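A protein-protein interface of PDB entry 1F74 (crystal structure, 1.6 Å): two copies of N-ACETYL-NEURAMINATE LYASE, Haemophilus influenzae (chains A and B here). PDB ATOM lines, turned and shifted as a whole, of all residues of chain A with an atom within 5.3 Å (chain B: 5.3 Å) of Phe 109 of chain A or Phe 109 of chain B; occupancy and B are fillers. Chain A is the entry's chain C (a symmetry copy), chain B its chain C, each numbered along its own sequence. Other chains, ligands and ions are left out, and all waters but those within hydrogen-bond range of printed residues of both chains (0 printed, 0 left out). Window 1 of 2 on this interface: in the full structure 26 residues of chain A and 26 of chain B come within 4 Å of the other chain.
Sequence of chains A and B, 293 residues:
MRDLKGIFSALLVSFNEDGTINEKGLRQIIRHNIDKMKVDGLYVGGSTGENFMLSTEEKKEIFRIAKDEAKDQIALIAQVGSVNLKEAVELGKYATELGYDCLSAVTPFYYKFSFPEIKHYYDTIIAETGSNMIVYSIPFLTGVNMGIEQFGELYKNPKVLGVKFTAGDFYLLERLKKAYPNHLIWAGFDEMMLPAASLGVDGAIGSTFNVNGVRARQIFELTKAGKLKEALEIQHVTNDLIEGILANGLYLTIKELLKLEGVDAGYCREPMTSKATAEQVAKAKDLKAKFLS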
ATOM      1  N   PHE A  52       0.092  -4.581 -15.289  1.00  0.00           N
ATOM      2  CA  PHE A  52      -0.767  -3.556 -14.704  1.00  0.00           C
ATOM      3  C   PHE A  52      -0.384  -2.140 -15.076  1.00  0.00           C
ATOM      4  O   PHE A  52      -1.190  -1.234 -14.826  1.00  0.00           O
ATOM      5  CB  PHE A  52      -0.888  -3.807 -13.187  1.00  0.00           C
ATOM      6  CG  PHE A  52      -1.441  -5.196 -12.928  1.00  0.00           C
ATOM      7  CD1 PHE A  52      -2.786  -5.452 -13.067  1.00  0.00           C
ATOM      8  CD2 PHE A  52      -0.588  -6.230 -12.563  1.00  0.00           C
ATOM      9  CE1 PHE A  52      -3.300  -6.728 -12.833  1.00  0.00           C
ATOM     10  CE2 PHE A  52      -1.088  -7.497 -12.333  1.00  0.00           C
ATOM     11  CZ  PHE A  52      -2.438  -7.744 -12.474  1.00  0.00           C
ATOM     12  N   SER A  82      -8.033  -7.677 -12.725  1.00  0.00           N
ATOM     13  CA  SER A  82      -8.008  -6.218 -12.778  1.00  0.00           C
ATOM     14  C   SER A  82      -8.887  -5.667 -11.676  1.00  0.00           C
ATOM     15  O   SER A  82      -9.759  -6.371 -11.176  1.00  0.00           O
ATOM     16  CB  SER A  82      -8.657  -5.842 -14.127  1.00  0.00           C
ATOM     17  OG  SER A  82      -8.744  -4.431 -14.285  1.00  0.00           O
ATOM     18  N   VAL A  83      -8.725  -4.370 -11.380  1.00  0.00           N
ATOM     19  CA  VAL A  83      -9.660  -3.712 -10.462  1.00  0.00           C
ATOM     20  C   VAL A  83     -10.976  -3.475 -11.200  1.00  0.00           C
ATOM     21  O   VAL A  83     -12.036  -3.359 -10.589  1.00  0.00           O
ATOM     22  CB  VAL A  83      -9.081  -2.394  -9.947  1.00  0.00           C
ATOM     23  CG1 VAL A  83     -10.002  -1.743  -8.928  1.00  0.00           C
ATOM     24  CG2 VAL A  83      -7.700  -2.613  -9.322  1.00  0.00           C
ATOM     25  N   VAL A 106      -5.637 -12.035 -10.522  1.00  0.00           N
ATOM     26  CA  VAL A 106      -5.269 -11.511  -9.209  1.00  0.00           C
ATOM     27  C   VAL A 106      -6.539 -11.100  -8.454  1.00  0.00           C
ATOM     28  O   VAL A 106      -7.584 -10.826  -9.046  1.00  0.00           O
ATOM     29  CB  VAL A 106      -4.379 -10.262  -9.361  1.00  0.00           C
ATOM     30  CG1 VAL A 106      -3.030 -10.636  -9.962  1.00  0.00           C
ATOM     31  CG2 VAL A 106      -5.066  -9.179 -10.186  1.00  0.00           C
ATOM     32  N   THR A 107      -6.415 -10.998  -7.126  1.00  0.00           N
ATOM     33  CA  THR A 107      -7.548 -10.482  -6.347  1.00  0.00           C
ATOM     34  C   THR A 107      -7.717  -9.018  -6.740  1.00  0.00           C
ATOM     35  O   THR A 107      -6.718  -8.332  -6.977  1.00  0.00           O
ATOM     36  CB  THR A 107      -7.118 -10.541  -4.868  1.00  0.00           C
ATOM     37  OG1 THR A 107      -6.309 -11.703  -4.650  1.00  0.00           O
ATOM     38  CG2 THR A 107      -8.332 -10.603  -3.958  1.00  0.00           C
ATOM     39  N   PRO A 108      -8.936  -8.527  -6.880  1.00  0.00           N
ATOM     40  CA  PRO A 108      -9.137  -7.103  -7.201  1.00  0.00           C
ATOM     41  C   PRO A 108      -8.438  -6.291  -6.112  1.00  0.00           C
ATOM     42  O   PRO A 108      -8.512  -6.630  -4.931  1.00  0.00           O
ATOM     43  CB  PRO A 108     -10.634  -6.957  -7.293  1.00  0.00           C
ATOM     44  CG  PRO A 108     -11.186  -8.075  -6.490  1.00  0.00           C
ATOM     45  CD  PRO A 108     -10.215  -9.234  -6.656  1.00  0.00           C
ATOM     46  N   PHE A 109      -7.727  -5.244  -6.528  1.00  0.00           N
ATOM     47  CA  PHE A 109      -6.868  -4.490  -5.615  1.00  0.00           C
ATOM     48  C   PHE A 109      -7.204  -3.021  -5.576  1.00  0.00           C
ATOM     49  O   PHE A 109      -8.319  -2.622  -5.912  1.00  0.00           O
ATOM     50  CB  PHE A 109      -5.407  -4.770  -5.985  1.00  0.00           C
ATOM     51  CG  PHE A 109      -5.036  -4.514  -7.413  1.00  0.00           C
ATOM     52  CD1 PHE A 109      -5.247  -5.478  -8.396  1.00  0.00           C
ATOM     53  CD2 PHE A 109      -4.481  -3.297  -7.793  1.00  0.00           C
ATOM     54  CE1 PHE A 109      -4.912  -5.221  -9.711  1.00  0.00           C
ATOM     55  CE2 PHE A 109      -4.140  -3.043  -9.103  1.00  0.00           C
ATOM     56  CZ  PHE A 109      -4.345  -4.011 -10.071  1.00  0.00           C
ATOM     57  N   TYR A 110      -6.312  -2.203  -5.027  1.00  0.00           N
ATOM     58  CA  TYR A 110      -6.538  -0.796  -4.817  1.00  0.00           C
ATOM     59  C   TYR A 110      -7.675  -0.640  -3.809  1.00  0.00           C
ATOM     60  O   TYR A 110      -7.418   0.292  -3.068  1.00  0.00           O
ATOM     61  CB  TYR A 110      -6.874   0.142  -5.974  1.00  0.00           C
ATOM     62  CG  TYR A 110      -6.918   1.601  -5.513  1.00  0.00           C
ATOM     63  CD1 TYR A 110      -5.740   2.329  -5.522  1.00  0.00           C
ATOM     64  CD2 TYR A 110      -8.067   2.205  -5.047  1.00  0.00           C
ATOM     65  CE1 TYR A 110      -5.713   3.645  -5.090  1.00  0.00           C
ATOM     66  CE2 TYR A 110      -8.058   3.520  -4.611  1.00  0.00           C
ATOM     67  CZ  TYR A 110      -6.877   4.230  -4.650  1.00  0.00           C
ATOM     68  OH  TYR A 110      -6.840   5.547  -4.229  1.00  0.00           O
ATOM     69  N   TYR A 111      -8.860  -1.171  -3.843  1.00  0.00           N
ATOM     70  CA  TYR A 111      -9.797  -1.015  -2.759  1.00  0.00           C
ATOM     71  C   TYR A 111      -9.684  -2.316  -1.953  1.00  0.00           C
ATOM     72  O   TYR A 111      -9.141  -3.302  -2.440  1.00  0.00           O
ATOM     73  CB  TYR A 111     -11.247  -0.908  -3.200  1.00  0.00           C
ATOM     74  CG  TYR A 111     -11.482   0.323  -4.036  1.00  0.00           C
ATOM     75  CD1 TYR A 111     -11.738   1.555  -3.456  1.00  0.00           C
ATOM     76  CD2 TYR A 111     -11.439   0.216  -5.418  1.00  0.00           C
ATOM     77  CE1 TYR A 111     -11.962   2.649  -4.265  1.00  0.00           C
ATOM     78  CE2 TYR A 111     -11.651   1.319  -6.226  1.00  0.00           C
ATOM     79  CZ  TYR A 111     -11.926   2.532  -5.631  1.00  0.00           C
ATOM     80  OH  TYR A 111     -12.137   3.640  -6.422  1.00  0.00           O
ATOM     81  N   PHE A 113     -11.572  -5.375  -0.737  1.00  0.00           N
ATOM     82  CA  PHE A 113     -12.828  -6.062  -1.057  1.00  0.00           C
ATOM     83  C   PHE A 113     -13.143  -7.110  -0.003  1.00  0.00           C
ATOM     84  O   PHE A 113     -12.216  -7.679   0.578  1.00  0.00           O
ATOM     85  CB  PHE A 113     -12.724  -6.665  -2.457  1.00  0.00           C
ATOM     86  CG  PHE A 113     -12.602  -5.614  -3.530  1.00  0.00           C
ATOM     87  CD1 PHE A 113     -13.737  -5.069  -4.086  1.00  0.00           C
ATOM     88  CD2 PHE A 113     -11.359  -5.185  -3.972  1.00  0.00           C
ATOM     89  CE1 PHE A 113     -13.644  -4.097  -5.069  1.00  0.00           C
ATOM     90  CE2 PHE A 113     -11.267  -4.207  -4.954  1.00  0.00           C
ATOM     91  CZ  PHE A 113     -12.409  -3.682  -5.520  1.00  0.00           C
ATOM     92  N   PHE B  52     -11.045   3.592  -9.911  1.00  0.00           N
ATOM     93  CA  PHE B  52     -10.127   2.536 -10.329  1.00  0.00           C
ATOM     94  C   PHE B  52     -10.812   1.284 -10.831  1.00  0.00           C
ATOM     95  O   PHE B  52     -10.125   0.442 -11.425  1.00  0.00           O
ATOM     96  CB  PHE B  52      -9.094   2.294  -9.209  1.00  0.00           C
ATOM     97  CG  PHE B  52      -8.345   3.577  -8.900  1.00  0.00           C
ATOM     98  CD1 PHE B  52      -7.333   4.013  -9.725  1.00  0.00           C
ATOM     99  CD2 PHE B  52      -8.687   4.334  -7.787  1.00  0.00           C
ATOM    100  CE1 PHE B  52      -6.643   5.193  -9.448  1.00  0.00           C
ATOM    101  CE2 PHE B  52      -8.011   5.506  -7.507  1.00  0.00           C
ATOM    102  CZ  PHE B  52      -6.998   5.935  -8.339  1.00  0.00           C
ATOM    103  N   SER B  82      -2.718   6.580 -11.895  1.00  0.00           N
ATOM    104  CA  SER B  82      -2.933   5.224 -12.392  1.00  0.00           C
ATOM    105  C   SER B  82      -1.638   4.447 -12.289  1.00  0.00           C
ATOM    106  O   SER B  82      -0.568   5.044 -12.218  1.00  0.00           O
ATOM    107  CB  SER B  82      -3.269   5.380 -13.890  1.00  0.00           C
ATOM    108  OG  SER B  82      -3.453   4.116 -14.516  1.00  0.00           O
ATOM    109  N   VAL B  83      -1.735   3.116 -12.397  1.00  0.00           N
ATOM    110  CA  VAL B  83      -0.517   2.304 -12.497  1.00  0.00           C
ATOM    111  C   VAL B  83       0.058   2.468 -13.902  1.00  0.00           C
ATOM    112  O   VAL B  83       1.251   2.280 -14.127  1.00  0.00           O
ATOM    113  CB  VAL B  83      -0.815   0.834 -12.200  1.00  0.00           C
ATOM    114  CG1 VAL B  83       0.452  -0.005 -12.216  1.00  0.00           C
ATOM    115  CG2 VAL B  83      -1.512   0.683 -10.844  1.00  0.00           C
ATOM    116  N   VAL B 106      -2.811   9.691  -7.435  1.00  0.00           N
ATOM    117  CA  VAL B 106      -2.375   8.733  -6.423  1.00  0.00           C
ATOM    118  C   VAL B 106      -0.963   8.245  -6.763  1.00  0.00           C
ATOM    119  O   VAL B 106      -0.519   8.296  -7.911  1.00  0.00           O
ATOM    120  CB  VAL B 106      -3.312   7.509  -6.406  1.00  0.00           C
ATOM    121  CG1 VAL B 106      -4.700   7.904  -5.917  1.00  0.00           C
ATOM    122  CG2 VAL B 106      -3.383   6.836  -7.772  1.00  0.00           C
ATOM    123  N   THR B 107      -0.277   7.704  -5.749  1.00  0.00           N
ATOM    124  CA  THR B 107       1.030   7.094  -6.025  1.00  0.00           C
ATOM    125  C   THR B 107       0.765   5.866  -6.888  1.00  0.00           C
ATOM    126  O   THR B 107      -0.246   5.185  -6.685  1.00  0.00           O
ATOM    127  CB  THR B 107       1.581   6.622  -4.664  1.00  0.00           C
ATOM    128  OG1 THR B 107       1.201   7.552  -3.644  1.00  0.00           O
ATOM    129  CG2 THR B 107       3.096   6.522  -4.705  1.00  0.00           C
ATOM    130  N   PRO B 108       1.592   5.585  -7.880  1.00  0.00           N
ATOM    131  CA  PRO B 108       1.400   4.375  -8.696  1.00  0.00           C
ATOM    132  C   PRO B 108       1.407   3.181  -7.743  1.00  0.00           C
ATOM    133  O   PRO B 108       2.211   3.125  -6.813  1.00  0.00           O
ATOM    134  CB  PRO B 108       2.516   4.435  -9.707  1.00  0.00           C
ATOM    135  CG  PRO B 108       3.560   5.287  -9.088  1.00  0.00           C
ATOM    136  CD  PRO B 108       2.820   6.320  -8.253  1.00  0.00           C
ATOM    137  N   PHE B 109       0.477   2.253  -7.962  1.00  0.00           N
ATOM    138  CA  PHE B 109       0.258   1.152  -7.023  1.00  0.00           C
ATOM    139  C   PHE B 109       0.384  -0.203  -7.671  1.00  0.00           C
ATOM    140  O   PHE B 109       1.022  -0.344  -8.714  1.00  0.00           O
ATOM    141  CB  PHE B 109      -1.091   1.371  -6.328  1.00  0.00           C
ATOM    142  CG  PHE B 109      -2.269   1.552  -7.235  1.00  0.00           C
ATOM    143  CD1 PHE B 109      -2.582   2.800  -7.769  1.00  0.00           C
ATOM    144  CD2 PHE B 109      -3.072   0.470  -7.576  1.00  0.00           C
ATOM    145  CE1 PHE B 109      -3.664   2.947  -8.614  1.00  0.00           C
ATOM    146  CE2 PHE B 109      -4.155   0.617  -8.413  1.00  0.00           C
ATOM    147  CZ  PHE B 109      -4.465   1.863  -8.931  1.00  0.00           C
ATOM    148  N   TYR B 110      -0.087  -1.249  -7.000  1.00  0.00           N
ATOM    149  CA  TYR B 110       0.060  -2.614  -7.438  1.00  0.00           C
ATOM    150  C   TYR B 110       1.548  -2.960  -7.431  1.00  0.00           C
ATOM    151  O   TYR B 110       1.684  -4.104  -7.037  1.00  0.00           O
ATOM    152  CB  TYR B 110      -0.471  -3.082  -8.790  1.00  0.00           C
ATOM    153  CG  TYR B 110      -0.323  -4.597  -8.951  1.00  0.00           C
ATOM    154  CD1 TYR B 110      -1.344  -5.410  -8.489  1.00  0.00           C
ATOM    155  CD2 TYR B 110       0.799  -5.188  -9.494  1.00  0.00           C
ATOM    156  CE1 TYR B 110      -1.255  -6.790  -8.583  1.00  0.00           C
ATOM    157  CE2 TYR B 110       0.906  -6.565  -9.595  1.00  0.00           C
ATOM    158  CZ  TYR B 110      -0.134  -7.352  -9.146  1.00  0.00           C
ATOM    159  OH  TYR B 110      -0.058  -8.730  -9.243  1.00  0.00           O
ATOM    160  N   TYR B 111       2.527  -2.317  -7.993  1.00  0.00           N
ATOM    161  CA  TYR B 111       3.901  -2.710  -7.811  1.00  0.00           C
ATOM    162  C   TYR B 111       4.440  -1.762  -6.731  1.00  0.00           C
ATOM    163  O   TYR B 111       3.829  -0.739  -6.444  1.00  0.00           O
ATOM    164  CB  TYR B 111       4.776  -2.505  -9.037  1.00  0.00           C
ATOM    165  CG  TYR B 111       4.324  -3.364 -10.189  1.00  0.00           C
ATOM    166  CD1 TYR B 111       4.736  -4.681 -10.316  1.00  0.00           C
ATOM    167  CD2 TYR B 111       3.474  -2.821 -11.140  1.00  0.00           C
ATOM    168  CE1 TYR B 111       4.307  -5.421 -11.398  1.00  0.00           C
ATOM    169  CE2 TYR B 111       3.035  -3.571 -12.216  1.00  0.00           C
ATOM    170  CZ  TYR B 111       3.473  -4.873 -12.339  1.00  0.00           C
ATOM    171  OH  TYR B 111       3.043  -5.634 -13.403  1.00  0.00           O
ATOM    172  N   PHE B 113       7.008   0.929  -5.980  1.00  0.00           N
ATOM    173  CA  PHE B 113       7.890   1.820  -6.744  1.00  0.00           C
ATOM    174  C   PHE B 113       8.889   2.497  -5.821  1.00  0.00           C
ATOM    175  O   PHE B 113       8.564   2.740  -4.656  1.00  0.00           O
ATOM    176  CB  PHE B 113       7.036   2.827  -7.512  1.00  0.00           C
ATOM    177  CG  PHE B 113       6.179   2.174  -8.565  1.00  0.00           C
ATOM    178  CD1 PHE B 113       6.686   1.970  -9.829  1.00  0.00           C
ATOM    179  CD2 PHE B 113       4.881   1.775  -8.283  1.00  0.00           C
ATOM    180  CE1 PHE B 113       5.915   1.365 -10.808  1.00  0.00           C
ATOM    181  CE2 PHE B 113       4.111   1.165  -9.264  1.00  0.00           C
ATOM    182  CZ  PHE B 113       4.619   0.983 -10.533  1.00  0.00           C
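Among the printed residues, merely in contact across the chains: Phe 52 of chain A with Val 83 of chain B, Phe 52 of chain A with Tyr 110 of chain B, Phe 52 of chain A with Tyr 111 of chain B, Val 83 of chain A with Phe 52 of chain B, Val 106 of chain A with Tyr 110 of chain B, Phe 109 of chain A with Phe 109 of chain B, Phe 109 of chain A with Tyr 110 of chain B, Tyr 110 of chain A with Phe 52 of chain B, Tyr 110 of chain A with Val 106 of chain B, Tyr 110 of chain A with Phe 109 of chain B and Tyr 111 of chain A with Phe 52 of chain B.
Of the 10 printed residues of chain B, 6 touch a printed residue of chain A.
Printed residues of chain B that touch a printed residue of chain A: Phe 52, Val 83, Val 106, Phe 109, Tyr 110 and Tyr 111.
Of the 10 printed residues of chain A, 6 touch a printed residue of chain B.
Among the printed residues, no Asp or Glu carboxylate lies within 4 Å of a Lys or Arg side-chain nitrogen of the other chain.
Phe 109 of chain A touches just these residues of chain B: Phe 109 (3.7 Å) and Tyr 110 (3.7 Å).
Printed residues of chain A within 4 Å of Val 106 of chain B: Tyr 110.
Pro 108 of chain B touches none of the printed residues of chain A.
Of chain A, only Phe 109 and Tyr 110 come within 4 Å of Phe 109 of chain B.
Of the printed residues of chain A, Tyr 111 of chain B touches Phe 52 (3.7 Å).
The nearest residue of chain A that does not touch Phe 109 of chain B is Val 83 of chain A (4.9 Å).
The nearest printed residue of chain B that does not touch Phe 52 of chain A is Ser 82 of chain B (5.8 Å).
Phe 52 of chain A touches Val 83 of chain B, and with the chains exchanged Val 83 of chain A touches Phe 52 of chain B.
Phe 52 of chain A touches Tyr 111 of chain B, and with the chains exchanged Tyr 111 of chain A touches Phe 52 of chain B.
Phe 109 of chain B touches its own counterpart, Phe 109 of chain A.
Phe 109 of chain A touches Tyr 110 of chain B, and with the chains exchanged Tyr 110 of chain A touches Phe 109 of chain B.
Of the 11 pairs that touch across the chains among the printed residues, 11 have their exchanged pair printed and touching as well.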
